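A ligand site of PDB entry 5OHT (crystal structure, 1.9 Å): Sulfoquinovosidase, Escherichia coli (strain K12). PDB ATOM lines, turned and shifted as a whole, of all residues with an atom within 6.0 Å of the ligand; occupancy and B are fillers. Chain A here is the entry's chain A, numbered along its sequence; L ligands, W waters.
Water W2 lies within hydrogen-bond range of an oxygen (O4) of the ligand (2.7 Å), the side-chain carboxylate (OD2) of Asp 504 (2.7 Å), the side-chain carboxylate (OD1) of Asp 472 (2.9 Å) and the indole nitrogen (NE1) of Trp 469 (3.1 Å). Water W1 lies within hydrogen-bond range of O of Lys 300 (2.8 Å), OH of Tyr 508 (2.8 Å), O1 of the ligand (2.9 Å) and NE2 of Gln 288 (3.2 Å).
N of Val 302 lies within hydrogen-bond range of O2 of the ligand (3.0 Å). OD2 of Asp 405 is in salt-bridge range of N1 of the ligand. SD of Met 403 lies close to O4 of the ligand (3.7 Å). NE2 of His 537 is in hydrogen-bond range of O4 of the ligand (2.9 Å). NE1 of Trp 304 is in hydrogen-bond range of O2 of the ligand. An oxygen (O5) of the ligand is in hydrogen-bond range of the side-chain amide oxygen (OE1) of Gln 288, at 2.6 Å. An oxygen (O3) of the ligand is in salt-bridge range of the guanidinium group (NH1) of Arg 301 (2.9 Å).
Merely in contact with the ligand: Asp 472, Tyr 508, Arg 455, Phe 406 and Tyr 333. Hydrophobic or aromatic side chains within 4 Å of the ligand: Val 302, Trp 304, Tyr 333, Met 403, Phe 406, Tyr 508 and His 537. The nearest printed residue that does not touch the ligand is Trp 469 (4.01 Å).
The side-chain hydroxyl (OH) of Tyr 333 lies within hydrogen-bond range of the side-chain amide nitrogen (ND2) of Asn 335. The side-chain carboxylate (OD2) of Asp 405 is in hydrogen-bond range of the side-chain hydroxyl (OH) of Tyr 333. The guanidinium group (NE) of Arg 455 lies within salt-bridge range of the side-chain carboxylate (OD1) of Asp 405. The side-chain carboxylate of Asp 472 is in salt-bridge range of the guanidinium group of Arg 455 (3.6 Å).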
ATOM      1  N   TRP A 286     -20.109  -1.951  24.649  1.00  0.00           N
ATOM      2  CA  TRP A 286     -20.322  -2.534  23.326  1.00  0.00           C
ATOM      3  C   TRP A 286     -19.669  -3.913  23.313  1.00  0.00           C
ATOM      4  O   TRP A 286     -18.436  -4.033  23.344  1.00  0.00           O
ATOM      5  CB  TRP A 286     -19.765  -1.626  22.188  1.00  0.00           C
ATOM      6  CG  TRP A 286     -19.788  -2.340  20.879  1.00  0.00           C
ATOM      7  CD1 TRP A 286     -20.879  -2.851  20.279  1.00  0.00           C
ATOM      8  CD2 TRP A 286     -18.669  -2.659  20.029  1.00  0.00           C
ATOM      9  NE1 TRP A 286     -20.541  -3.487  19.122  1.00  0.00           N
ATOM     10  CE2 TRP A 286     -19.179  -3.391  18.937  1.00  0.00           C
ATOM     11  CE3 TRP A 286     -17.303  -2.398  20.091  1.00  0.00           C
ATOM     12  CZ2 TRP A 286     -18.351  -3.878  17.910  1.00  0.00           C
ATOM     13  CZ3 TRP A 286     -16.478  -2.887  19.084  1.00  0.00           C
ATOM     14  CH2 TRP A 286     -17.018  -3.636  18.005  1.00  0.00           C
ATOM     15  N   GLN A 288     -19.524  -7.218  21.154  1.00  0.00           N
ATOM     16  CA  GLN A 288     -19.873  -7.822  19.835  1.00  0.00           C
ATOM     17  C   GLN A 288     -20.149  -9.351  19.959  1.00  0.00           C
ATOM     18  O   GLN A 288     -20.841  -9.936  19.110  1.00  0.00           O
ATOM     19  CB  GLN A 288     -18.781  -7.557  18.808  1.00  0.00           C
ATOM     20  CG  GLN A 288     -17.400  -8.095  19.059  1.00  0.00           C
ATOM     21  CD  GLN A 288     -16.479  -7.985  17.828  1.00  0.00           C
ATOM     22  OE1 GLN A 288     -16.751  -7.222  16.907  1.00  0.00           O
ATOM     23  NE2 GLN A 288     -15.347  -8.727  17.846  1.00  0.00           N
ATOM     24  N   PHE A 298      -7.492 -15.895  12.031  1.00  0.00           N
ATOM     25  CA  PHE A 298      -7.484 -14.430  12.057  1.00  0.00           C
ATOM     26  C   PHE A 298      -7.440 -13.921  13.508  1.00  0.00           C
ATOM     27  O   PHE A 298      -6.764 -12.902  13.806  1.00  0.00           O
ATOM     28  CB  PHE A 298      -8.714 -13.898  11.273  1.00  0.00           C
ATOM     29  CG  PHE A 298      -8.764 -12.396  11.169  1.00  0.00           C
ATOM     30  CD1 PHE A 298      -7.809 -11.740  10.421  1.00  0.00           C
ATOM     31  CD2 PHE A 298      -9.806 -11.669  11.716  1.00  0.00           C
ATOM     32  CE1 PHE A 298      -7.867 -10.369  10.225  1.00  0.00           C
ATOM     33  CE2 PHE A 298      -9.855 -10.298  11.552  1.00  0.00           C
ATOM     34  CZ  PHE A 298      -8.881  -9.643  10.858  1.00  0.00           C
ATOM     35  N   LYS A 300     -10.008 -13.707  17.288  1.00  0.00           N
ATOM     36  CA  LYS A 300     -11.319 -13.861  17.845  1.00  0.00           C
ATOM     37  C   LYS A 300     -12.415 -13.139  17.067  1.00  0.00           C
ATOM     38  O   LYS A 300     -12.418 -11.904  16.993  1.00  0.00           O
ATOM     39  CB  LYS A 300     -11.261 -13.473  19.320  1.00  0.00           C
ATOM     40  CG  LYS A 300     -12.570 -13.439  20.084  1.00  0.00           C
ATOM     41  CD  LYS A 300     -12.266 -13.710  21.566  1.00  0.00           C
ATOM     42  CE  LYS A 300     -12.953 -12.789  22.476  1.00  0.00           C
ATOM     43  NZ  LYS A 300     -12.662 -13.159  23.918  1.00  0.00           N
ATOM     44  N   ARG A 301     -13.345 -13.920  16.507  1.00  0.00           N
ATOM     45  CA  ARG A 301     -14.483 -13.401  15.738  1.00  0.00           C
ATOM     46  C   ARG A 301     -15.839 -13.638  16.423  1.00  0.00           C
ATOM     47  O   ARG A 301     -15.949 -14.354  17.472  1.00  0.00           O
ATOM     48  CB  ARG A 301     -14.432 -13.966  14.310  1.00  0.00           C
ATOM     49  CG  ARG A 301     -13.062 -13.801  13.663  1.00  0.00           C
ATOM     50  CD  ARG A 301     -12.997 -13.959  12.115  1.00  0.00           C
ATOM     51  NE  ARG A 301     -13.887 -13.013  11.401  1.00  0.00           N
ATOM     52  CZ  ARG A 301     -14.108 -13.056  10.095  1.00  0.00           C
ATOM     53  NH1 ARG A 301     -14.920 -12.177   9.574  1.00  0.00           N
ATOM     54  NH2 ARG A 301     -13.532 -14.001   9.285  1.00  0.00           N
ATOM     55  N   VAL A 302     -16.885 -13.023  15.892  1.00  0.00           N
ATOM     56  CA  VAL A 302     -18.217 -13.207  16.422  1.00  0.00           C
ATOM     57  C   VAL A 302     -18.851 -14.502  15.796  1.00  0.00           C
ATOM     58  O   VAL A 302     -18.518 -14.892  14.667  1.00  0.00           O
ATOM     59  CB  VAL A 302     -19.096 -12.008  16.065  1.00  0.00           C
ATOM     60  CG1 VAL A 302     -20.509 -12.198  16.571  1.00  0.00           C
ATOM     61  CG2 VAL A 302     -18.462 -10.708  16.610  1.00  0.00           C
ATOM     62  N   MET A 303     -19.750 -15.138  16.546  1.00  0.00           N
ATOM     63  CA  MET A 303     -20.593 -16.248  16.028  1.00  0.00           C
ATOM     64  C   MET A 303     -21.779 -15.657  15.286  1.00  0.00           C
ATOM     65  O   MET A 303     -22.628 -15.044  15.941  1.00  0.00           O
ATOM     66  CB  MET A 303     -21.111 -17.187  17.160  1.00  0.00           C
ATOM     67  CG  MET A 303     -21.975 -18.354  16.624  1.00  0.00           C
ATOM     68  SD  MET A 303     -21.246 -19.280  15.221  1.00  0.00           S
ATOM     69  CE  MET A 303     -19.888 -20.082  15.989  1.00  0.00           C
ATOM     70  N   TRP A 304     -21.836 -15.819  13.970  1.00  0.00           N
ATOM     71  CA  TRP A 304     -22.856 -15.102  13.176  1.00  0.00           C
ATOM     72  C   TRP A 304     -24.208 -15.815  13.216  1.00  0.00           C
ATOM     73  O   TRP A 304     -24.682 -16.355  12.185  1.00  0.00           O
ATOM     74  CB  TRP A 304     -22.398 -14.905  11.714  1.00  0.00           C
ATOM     75  CG  TRP A 304     -21.136 -14.022  11.527  1.00  0.00           C
ATOM     76  CD1 TRP A 304     -20.344 -13.455  12.506  1.00  0.00           C
ATOM     77  CD2 TRP A 304     -20.552 -13.631  10.265  1.00  0.00           C
ATOM     78  NE1 TRP A 304     -19.327 -12.717  11.928  1.00  0.00           N
ATOM     79  CE2 TRP A 304     -19.421 -12.822  10.548  1.00  0.00           C
ATOM     80  CE3 TRP A 304     -20.892 -13.884   8.922  1.00  0.00           C
ATOM     81  CZ2 TRP A 304     -18.658 -12.257   9.556  1.00  0.00           C
ATOM     82  CZ3 TRP A 304     -20.086 -13.335   7.905  1.00  0.00           C
ATOM     83  CH2 TRP A 304     -18.977 -12.545   8.234  1.00  0.00           C
ATOM     84  N   TYR A 333     -24.183  -6.378  18.092  1.00  0.00           N
ATOM     85  CA  TYR A 333     -23.541  -6.584  16.766  1.00  0.00           C
ATOM     86  C   TYR A 333     -24.488  -7.399  15.885  1.00  0.00           C
ATOM     87  O   TYR A 333     -24.986  -8.461  16.319  1.00  0.00           O
ATOM     88  CB  TYR A 333     -22.176  -7.310  16.920  1.00  0.00           C
ATOM     89  CG  TYR A 333     -21.476  -7.631  15.607  1.00  0.00           C
ATOM     90  CD1 TYR A 333     -21.873  -8.731  14.824  1.00  0.00           C
ATOM     91  CD2 TYR A 333     -20.516  -6.757  15.038  1.00  0.00           C
ATOM     92  CE1 TYR A 333     -21.307  -8.969  13.574  1.00  0.00           C
ATOM     93  CE2 TYR A 333     -19.972  -7.005  13.794  1.00  0.00           C
ATOM     94  CZ  TYR A 333     -20.385  -8.101  13.050  1.00  0.00           C
ATOM     95  OH  TYR A 333     -19.844  -8.351  11.825  1.00  0.00           O
ATOM     96  N   ASN A 335     -24.845  -8.406  11.254  1.00  0.00           N
ATOM     97  CA  ASN A 335     -24.566  -8.230   9.830  1.00  0.00           C
ATOM     98  C   ASN A 335     -25.635  -8.962   9.024  1.00  0.00           C
ATOM     99  O   ASN A 335     -26.459  -9.703   9.616  1.00  0.00           O
ATOM    100  CB  ASN A 335     -23.078  -8.539   9.475  1.00  0.00           C
ATOM    101  CG  ASN A 335     -22.764 -10.019   9.394  1.00  0.00           C
ATOM    102  OD1 ASN A 335     -23.498 -10.792   8.788  1.00  0.00           O
ATOM    103  ND2 ASN A 335     -21.623 -10.415  10.009  1.00  0.00           N
ATOM    104  N   MET A 403     -23.344  -2.227  16.323  1.00  0.00           N
ATOM    105  CA  MET A 403     -22.627  -2.242  15.046  1.00  0.00           C
ATOM    106  C   MET A 403     -23.444  -2.987  14.019  1.00  0.00           C
ATOM    107  O   MET A 403     -23.819  -4.148  14.265  1.00  0.00           O
ATOM    108  CB  MET A 403     -21.267  -2.936  15.251  1.00  0.00           C
ATOM    109  CG  MET A 403     -20.359  -2.940  13.989  1.00  0.00           C
ATOM    110  SD  MET A 403     -18.709  -3.663  14.203  1.00  0.00           S
ATOM    111  CE  MET A 403     -17.780  -2.280  14.828  1.00  0.00           C
ATOM    112  N   ASP A 405     -22.768  -4.190  10.560  1.00  0.00           N
ATOM    113  CA  ASP A 405     -21.522  -4.388   9.823  1.00  0.00           C
ATOM    114  C   ASP A 405     -21.694  -4.934   8.418  1.00  0.00           C
ATOM    115  O   ASP A 405     -22.778  -5.371   8.048  1.00  0.00           O
ATOM    116  CB  ASP A 405     -20.690  -5.334  10.689  1.00  0.00           C
ATOM    117  CG  ASP A 405     -19.212  -5.369  10.373  1.00  0.00           C
ATOM    118  OD1 ASP A 405     -18.681  -4.529   9.643  1.00  0.00           O
ATOM    119  OD2 ASP A 405     -18.558  -6.264  10.894  1.00  0.00           O
ATOM    120  N   PHE A 406     -20.611  -4.940   7.645  1.00  0.00           N
ATOM    121  CA  PHE A 406     -20.550  -5.544   6.298  1.00  0.00           C
ATOM    122  C   PHE A 406     -21.569  -4.915   5.304  1.00  0.00           C
ATOM    123  O   PHE A 406     -21.974  -3.778   5.496  1.00  0.00           O
ATOM    124  CB  PHE A 406     -20.658  -7.102   6.349  1.00  0.00           C
ATOM    125  CG  PHE A 406     -19.449  -7.761   6.957  1.00  0.00           C
ATOM    126  CD1 PHE A 406     -18.340  -8.119   6.143  1.00  0.00           C
ATOM    127  CD2 PHE A 406     -19.404  -8.094   8.307  1.00  0.00           C
ATOM    128  CE1 PHE A 406     -17.239  -8.743   6.694  1.00  0.00           C
ATOM    129  CE2 PHE A 406     -18.294  -8.753   8.867  1.00  0.00           C
ATOM    130  CZ  PHE A 406     -17.209  -9.057   8.073  1.00  0.00           C
ATOM    131  N   ARG A 455     -20.267   0.678   8.481  1.00  0.00           N
ATOM    132  CA  ARG A 455     -19.002   0.972   7.753  1.00  0.00           C
ATOM    133  C   ARG A 455     -19.212   1.069   6.245  1.00  0.00           C
ATOM    134  O   ARG A 455     -18.493   1.831   5.584  1.00  0.00           O
ATOM    135  CB  ARG A 455     -17.890  -0.025   8.115  1.00  0.00           C
ATOM    136  CG  ARG A 455     -18.013  -1.404   7.464  1.00  0.00           C
ATOM    137  CD  ARG A 455     -16.872  -2.395   7.750  1.00  0.00           C
ATOM    138  NE  ARG A 455     -16.951  -3.555   6.837  1.00  0.00           N
ATOM    139  CZ  ARG A 455     -16.084  -4.610   6.876  1.00  0.00           C
ATOM    140  NH1 ARG A 455     -15.112  -4.634   7.794  1.00  0.00           N
ATOM    141  NH2 ARG A 455     -16.182  -5.603   5.982  1.00  0.00           N
ATOM    142  N   TRP A 469     -18.953   4.698  10.915  1.00  0.00           N
ATOM    143  CA  TRP A 469     -17.609   4.610  11.457  1.00  0.00           C
ATOM    144  C   TRP A 469     -16.671   4.219  10.294  1.00  0.00           C
ATOM    145  O   TRP A 469     -17.118   3.697   9.268  1.00  0.00           O
ATOM    146  CB  TRP A 469     -17.532   3.695  12.718  1.00  0.00           C
ATOM    147  CG  TRP A 469     -16.993   2.265  12.529  1.00  0.00           C
ATOM    148  CD1 TRP A 469     -15.722   1.845  12.768  1.00  0.00           C
ATOM    149  CD2 TRP A 469     -17.716   1.063  12.107  1.00  0.00           C
ATOM    150  NE1 TRP A 469     -15.580   0.528  12.525  1.00  0.00           N
ATOM    151  CE2 TRP A 469     -16.753   0.002  12.062  1.00  0.00           C
ATOM    152  CE3 TRP A 469     -19.015   0.790  11.731  1.00  0.00           C
ATOM    153  CZ2 TRP A 469     -17.087  -1.322  11.702  1.00  0.00           C
ATOM    154  CZ3 TRP A 469     -19.354  -0.526  11.360  1.00  0.00           C
ATOM    155  CH2 TRP A 469     -18.364  -1.565  11.351  1.00  0.00           C
ATOM    156  N   ASP A 472     -12.151  -0.764   9.332  1.00  0.00           N
ATOM    157  CA  ASP A 472     -10.910  -1.351   9.850  1.00  0.00           C
ATOM    158  C   ASP A 472      -9.611  -0.605   9.385  1.00  0.00           C
ATOM    159  O   ASP A 472      -9.188  -0.720   8.220  1.00  0.00           O
ATOM    160  CB  ASP A 472     -10.731  -2.840   9.418  1.00  0.00           C
ATOM    161  CG  ASP A 472     -11.946  -3.735   9.775  1.00  0.00           C
ATOM    162  OD1 ASP A 472     -12.981  -3.264  10.336  1.00  0.00           O
ATOM    163  OD2 ASP A 472     -11.847  -4.925   9.473  1.00  0.00           O
ATOM    164  N   ASP A 504     -12.762   3.513  15.410  1.00  0.00           N
ATOM    165  CA  ASP A 504     -12.368   2.610  16.516  1.00  0.00           C
ATOM    166  C   ASP A 504     -11.205   3.319  17.256  1.00  0.00           C
ATOM    167  O   ASP A 504     -10.143   3.558  16.640  1.00  0.00           O
ATOM    168  CB  ASP A 504     -11.802   1.292  16.013  1.00  0.00           C
ATOM    169  CG  ASP A 504     -12.792   0.438  15.233  1.00  0.00           C
ATOM    170  OD1 ASP A 504     -13.965   0.319  15.654  1.00  0.00           O
ATOM    171  OD2 ASP A 504     -12.380  -0.126  14.187  1.00  0.00           O
ATOM    172  N   TYR A 508      -8.055  -1.392  14.529  1.00  0.00           N
ATOM    173  CA  TYR A 508      -8.571  -2.768  14.550  1.00  0.00           C
ATOM    174  C   TYR A 508      -7.610  -3.872  14.114  1.00  0.00           C
ATOM    175  O   TYR A 508      -7.345  -4.835  14.897  1.00  0.00           O
ATOM    176  CB  TYR A 508      -9.817  -2.860  13.687  1.00  0.00           C
ATOM    177  CG  TYR A 508     -10.398  -4.260  13.644  1.00  0.00           C
ATOM    178  CD1 TYR A 508     -11.043  -4.791  14.762  1.00  0.00           C
ATOM    179  CD2 TYR A 508     -10.233  -5.086  12.503  1.00  0.00           C
ATOM    180  CE1 TYR A 508     -11.514  -6.090  14.736  1.00  0.00           C
ATOM    181  CE2 TYR A 508     -10.755  -6.397  12.487  1.00  0.00           C
ATOM    182  CZ  TYR A 508     -11.354  -6.888  13.607  1.00  0.00           C
ATOM    183  OH  TYR A 508     -11.863  -8.168  13.585  1.00  0.00           O
ATOM    184  N   HIS A 537     -12.272  -0.417  20.776  1.00  0.00           N
ATOM    185  CA  HIS A 537     -12.291  -1.764  20.135  1.00  0.00           C
ATOM    186  C   HIS A 537     -11.089  -2.569  20.660  1.00  0.00           C
ATOM    187  O   HIS A 537      -9.996  -2.067  20.752  1.00  0.00           O
ATOM    188  CB  HIS A 537     -12.223  -1.643  18.557  1.00  0.00           C
ATOM    189  CG  HIS A 537     -12.801  -2.813  17.807  1.00  0.00           C
ATOM    190  ND1 HIS A 537     -12.695  -4.122  18.251  1.00  0.00           N
ATOM    191  CD2 HIS A 537     -13.553  -2.855  16.670  1.00  0.00           C
ATOM    192  CE1 HIS A 537     -13.389  -4.908  17.437  1.00  0.00           C
ATOM    193  NE2 HIS A 537     -13.947  -4.164  16.473  1.00  0.00           N
HETATM  194  O1  LIG L   1     -14.732 -10.826  13.210  1.00  0.00           O
HETATM  195  S1  LIG L   1     -16.094 -10.505  12.926  1.00  0.00           S
HETATM  196  O2  LIG L   1     -17.154 -11.287  13.443  1.00  0.00           O
HETATM  197  O3  LIG L   1     -16.307 -10.517  11.441  1.00  0.00           O
HETATM  198  C1  LIG L   1     -16.442  -8.832  13.443  1.00  0.00           C
HETATM  199  C2  LIG L   1     -15.438  -7.741  13.031  1.00  0.00           C
HETATM  200  C3  LIG L   1     -15.385  -7.533  11.528  1.00  0.00           C
HETATM  201  N1  LIG L   1     -15.940  -6.291  10.968  1.00  0.00           N
HETATM  202  C4  LIG L   1     -15.386  -5.074  11.594  1.00  0.00           C
HETATM  203  C5  LIG L   1     -14.885  -5.273  13.025  1.00  0.00           C
HETATM  204  O4  LIG L   1     -15.031  -4.075  13.768  1.00  0.00           O
HETATM  205  C6  LIG L   1     -15.615  -6.396  13.759  1.00  0.00           C
HETATM  206  O5  LIG L   1     -15.072  -6.499  15.072  1.00  0.00           O
HETATM  207  O   HOH W   1     -13.314  -9.685  15.505  1.00  0.00           O
HETATM  208  O   HOH W   2     -13.741  -1.978  12.778  1.00  0.00           O
